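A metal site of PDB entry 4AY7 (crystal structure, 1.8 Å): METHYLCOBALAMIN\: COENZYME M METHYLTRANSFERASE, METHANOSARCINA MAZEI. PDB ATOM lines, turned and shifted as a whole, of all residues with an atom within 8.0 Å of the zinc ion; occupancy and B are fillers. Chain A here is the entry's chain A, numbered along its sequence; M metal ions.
ND1 of His 246 lies within hydrogen-bond range of OG of Ser 267 (2.8 Å).
The backbone NH (N) of Asp 211 is in hydrogen-bond range of the backbone carbonyl oxygen (O) of His 246 (2.9 Å).
OG1 of Thr 37 is in hydrogen-bond range of O of Cys 325 (2.8 Å).
The side-chain hydroxyl of Ser 294 lies within hydrogen-bond range of the backbone carbonyl oxygen of Cys 325 (3.0 Å).
The nearest printed residue that does not touch the zinc ion is Glu 269 (4.2 Å).
The zinc ion is bound by NE2 of His 246 (2.2 Å), SG of Cys 248 (2.4 Å) and SG of Cys 325 (2.5 Å).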
ATOM      1  N   THR A  37       9.403 -17.505 -21.347  1.00  0.00           N
ATOM      2  CA  THR A  37       8.735 -16.877 -20.244  1.00  0.00           C
ATOM      3  C   THR A  37       7.221 -16.860 -20.632  1.00  0.00           C
ATOM      4  O   THR A  37       6.867 -17.234 -21.737  1.00  0.00           O
ATOM      5  CB  THR A  37       9.272 -15.443 -20.092  1.00  0.00           C
ATOM      6  OG1 THR A  37       9.169 -14.786 -21.354  1.00  0.00           O
ATOM      7  CG2 THR A  37      10.781 -15.490 -19.664  1.00  0.00           C
ATOM      8  N   LEU A  84       3.560 -18.259 -11.802  1.00  0.00           N
ATOM      9  CA  LEU A  84       4.640 -18.779 -10.986  1.00  0.00           C
ATOM     10  C   LEU A  84       4.138 -19.303  -9.627  1.00  0.00           C
ATOM     11  O   LEU A  84       4.779 -19.084  -8.598  1.00  0.00           O
ATOM     12  CB  LEU A  84       5.670 -17.666 -10.785  1.00  0.00           C
ATOM     13  CG  LEU A  84       6.336 -17.334 -12.119  1.00  0.00           C
ATOM     14  CD1 LEU A  84       7.254 -16.122 -11.833  1.00  0.00           C
ATOM     15  CD2 LEU A  84       7.039 -18.574 -12.694  1.00  0.00           C
ATOM     16  N   ALA A 210      11.817 -19.588 -13.516  1.00  0.00           N
ATOM     17  CA  ALA A 210      11.874 -18.180 -13.274  1.00  0.00           C
ATOM     18  C   ALA A 210      12.093 -18.007 -11.798  1.00  0.00           C
ATOM     19  O   ALA A 210      11.277 -18.462 -10.998  1.00  0.00           O
ATOM     20  CB  ALA A 210      10.613 -17.486 -13.772  1.00  0.00           C
ATOM     21  N   ASP A 211      13.172 -17.368 -11.383  1.00  0.00           N
ATOM     22  CA  ASP A 211      13.472 -17.297 -10.031  1.00  0.00           C
ATOM     23  C   ASP A 211      13.746 -15.881  -9.569  1.00  0.00           C
ATOM     24  O   ASP A 211      14.848 -15.549  -9.209  1.00  0.00           O
ATOM     25  CB  ASP A 211      14.683 -18.219  -9.724  1.00  0.00           C
ATOM     26  CG  ASP A 211      14.541 -18.979  -8.368  1.00  0.00           C
ATOM     27  OD1 ASP A 211      13.800 -18.453  -7.515  1.00  0.00           O
ATOM     28  OD2 ASP A 211      15.222 -20.043  -8.143  1.00  0.00           O
ATOM     29  N   PRO A 212      12.715 -15.055  -9.545  1.00  0.00           N
ATOM     30  CA  PRO A 212      12.947 -13.648  -9.213  1.00  0.00           C
ATOM     31  C   PRO A 212      13.532 -13.358  -7.840  1.00  0.00           C
ATOM     32  O   PRO A 212      14.205 -12.363  -7.701  1.00  0.00           O
ATOM     33  CB  PRO A 212      11.559 -13.047  -9.345  1.00  0.00           C
ATOM     34  CG  PRO A 212      10.625 -14.199  -9.142  1.00  0.00           C
ATOM     35  CD  PRO A 212      11.336 -15.261  -9.942  1.00  0.00           C
ATOM     36  N   HIS A 246      15.897 -18.161 -15.680  1.00  0.00           N
ATOM     37  CA  HIS A 246      15.524 -16.773 -15.871  1.00  0.00           C
ATOM     38  C   HIS A 246      15.528 -16.046 -14.559  1.00  0.00           C
ATOM     39  O   HIS A 246      14.748 -16.453 -13.652  1.00  0.00           O
ATOM     40  CB  HIS A 246      14.196 -16.704 -16.553  1.00  0.00           C
ATOM     41  CG  HIS A 246      13.677 -15.296 -16.622  1.00  0.00           C
ATOM     42  ND1 HIS A 246      13.975 -14.471 -17.611  1.00  0.00           N
ATOM     43  CD2 HIS A 246      12.909 -14.545 -15.737  1.00  0.00           C
ATOM     44  CE1 HIS A 246      13.500 -13.244 -17.375  1.00  0.00           C
ATOM     45  NE2 HIS A 246      12.785 -13.298 -16.273  1.00  0.00           N
ATOM     46  N   ILE A 247      16.324 -14.996 -14.394  1.00  0.00           N
ATOM     47  CA  ILE A 247      16.317 -14.241 -13.127  1.00  0.00           C
ATOM     48  C   ILE A 247      16.124 -12.812 -13.540  1.00  0.00           C
ATOM     49  O   ILE A 247      16.898 -12.277 -14.343  1.00  0.00           O
ATOM     50  CB  ILE A 247      17.591 -14.399 -12.259  1.00  0.00           C
ATOM     51  CG1 ILE A 247      17.743 -15.831 -11.738  1.00  0.00           C
ATOM     52  CG2 ILE A 247      17.600 -13.446 -11.034  1.00  0.00           C
ATOM     53  CD1 ILE A 247      19.022 -16.047 -10.880  1.00  0.00           C
ATOM     54  N   CYS A 248      15.011 -12.244 -13.081  1.00  0.00           N
ATOM     55  CA  CYS A 248      14.589 -10.921 -13.523  1.00  0.00           C
ATOM     56  C   CYS A 248      15.552  -9.940 -12.884  1.00  0.00           C
ATOM     57  O   CYS A 248      16.126 -10.202 -11.831  1.00  0.00           O
ATOM     58  CB  CYS A 248      13.197 -10.534 -12.933  1.00  0.00           C
ATOM     59  SG  CYS A 248      11.935 -11.807 -12.944  1.00  0.00           S
ATOM     60  N   GLY A 249      15.615  -8.744 -13.429  1.00  0.00           N
ATOM     61  CA  GLY A 249      16.249  -7.650 -12.717  1.00  0.00           C
ATOM     62  C   GLY A 249      17.691  -7.414 -13.175  1.00  0.00           C
ATOM     63  O   GLY A 249      18.134  -7.974 -14.158  1.00  0.00           O
ATOM     64  N   SER A 267      18.209 -16.823 -19.417  1.00  0.00           N
ATOM     65  CA  SER A 267      17.199 -15.868 -19.969  1.00  0.00           C
ATOM     66  C   SER A 267      17.347 -14.633 -19.157  1.00  0.00           C
ATOM     67  O   SER A 267      17.161 -14.654 -17.927  1.00  0.00           O
ATOM     68  CB  SER A 267      15.820 -16.427 -19.864  1.00  0.00           C
ATOM     69  OG  SER A 267      14.809 -15.449 -20.051  1.00  0.00           O
ATOM     70  N   VAL A 268      17.568 -13.518 -19.857  1.00  0.00           N
ATOM     71  CA  VAL A 268      17.888 -12.259 -19.227  1.00  0.00           C
ATOM     72  C   VAL A 268      17.062 -11.090 -19.851  1.00  0.00           C
ATOM     73  O   VAL A 268      16.604 -11.170 -20.971  1.00  0.00           O
ATOM     74  CB  VAL A 268      19.337 -11.826 -19.470  1.00  0.00           C
ATOM     75  CG1 VAL A 268      20.266 -12.808 -18.781  1.00  0.00           C
ATOM     76  CG2 VAL A 268      19.634 -11.747 -20.990  1.00  0.00           C
ATOM     77  N   GLU A 269      16.893 -10.074 -19.034  1.00  0.00           N
ATOM     78  CA  GLU A 269      16.173  -8.889 -19.433  1.00  0.00           C
ATOM     79  C   GLU A 269      17.106  -7.944 -20.131  1.00  0.00           C
ATOM     80  O   GLU A 269      18.311  -7.949 -19.949  1.00  0.00           O
ATOM     81  CB  GLU A 269      15.650  -8.171 -18.182  1.00  0.00           C
ATOM     82  CG  GLU A 269      14.425  -8.795 -17.556  1.00  0.00           C
ATOM     83  CD  GLU A 269      13.670  -7.781 -16.699  1.00  0.00           C
ATOM     84  OE1 GLU A 269      14.041  -7.652 -15.512  1.00  0.00           O
ATOM     85  OE2 GLU A 269      12.700  -7.126 -17.220  1.00  0.00           O
ATOM     86  N   LYS A 271      17.452  -4.903 -19.437  1.00  0.00           N
ATOM     87  CA  LYS A 271      18.015  -4.043 -18.388  1.00  0.00           C
ATOM     88  C   LYS A 271      19.490  -4.190 -18.223  1.00  0.00           C
ATOM     89  O   LYS A 271      20.202  -3.207 -18.003  1.00  0.00           O
ATOM     90  CB  LYS A 271      17.406  -4.420 -17.015  1.00  0.00           C
ATOM     91  CG  LYS A 271      16.232  -3.616 -16.518  1.00  0.00           C
ATOM     92  CD  LYS A 271      15.755  -4.190 -15.176  1.00  0.00           C
ATOM     93  CE  LYS A 271      14.245  -3.958 -15.018  1.00  0.00           C
ATOM     94  NZ  LYS A 271      13.525  -4.984 -15.834  1.00  0.00           N
ATOM     95  N   SER A 294      10.177  -6.623 -22.411  1.00  0.00           N
ATOM     96  CA  SER A 294       8.705  -6.806 -22.368  1.00  0.00           C
ATOM     97  C   SER A 294       7.895  -5.516 -22.052  1.00  0.00           C
ATOM     98  O   SER A 294       6.955  -5.206 -22.745  1.00  0.00           O
ATOM     99  CB  SER A 294       8.287  -7.911 -21.372  1.00  0.00           C
ATOM    100  OG  SER A 294       8.776  -9.164 -21.909  1.00  0.00           O
ATOM    101  N   PRO A 323      11.462 -12.606 -25.725  1.00  0.00           N
ATOM    102  CA  PRO A 323      11.204 -11.507 -24.810  1.00  0.00           C
ATOM    103  C   PRO A 323      12.196 -11.582 -23.623  1.00  0.00           C
ATOM    104  O   PRO A 323      12.555 -12.676 -23.176  1.00  0.00           O
ATOM    105  CB  PRO A 323       9.768 -11.765 -24.361  1.00  0.00           C
ATOM    106  CG  PRO A 323       9.174 -12.554 -25.495  1.00  0.00           C
ATOM    107  CD  PRO A 323      10.275 -13.438 -25.941  1.00  0.00           C
ATOM    108  N   GLY A 324      12.519 -10.445 -23.040  1.00  0.00           N
ATOM    109  CA  GLY A 324      13.351 -10.444 -21.890  1.00  0.00           C
ATOM    110  C   GLY A 324      12.682 -10.964 -20.610  1.00  0.00           C
ATOM    111  O   GLY A 324      13.345 -11.450 -19.751  1.00  0.00           O
ATOM    112  N   CYS A 325      11.385 -10.810 -20.475  1.00  0.00           N
ATOM    113  CA  CYS A 325      10.661 -11.226 -19.277  1.00  0.00           C
ATOM    114  C   CYS A 325       9.346 -11.805 -19.775  1.00  0.00           C
ATOM    115  O   CYS A 325       9.167 -11.970 -20.980  1.00  0.00           O
ATOM    116  CB  CYS A 325      10.471 -10.059 -18.295  1.00  0.00           C
ATOM    117  SG  CYS A 325      10.004 -10.730 -16.688  1.00  0.00           S
ATOM    118  N   GLY A 326       8.434 -12.178 -18.871  1.00  0.00           N
ATOM    119  CA  GLY A 326       7.100 -12.605 -19.344  1.00  0.00           C
ATOM    120  C   GLY A 326       6.492 -11.505 -20.239  1.00  0.00           C
ATOM    121  O   GLY A 326       6.727 -10.290 -20.048  1.00  0.00           O
HETATM  122 ZN    ZN M   1      12.022 -11.423 -15.322  1.00  0.00          ZN
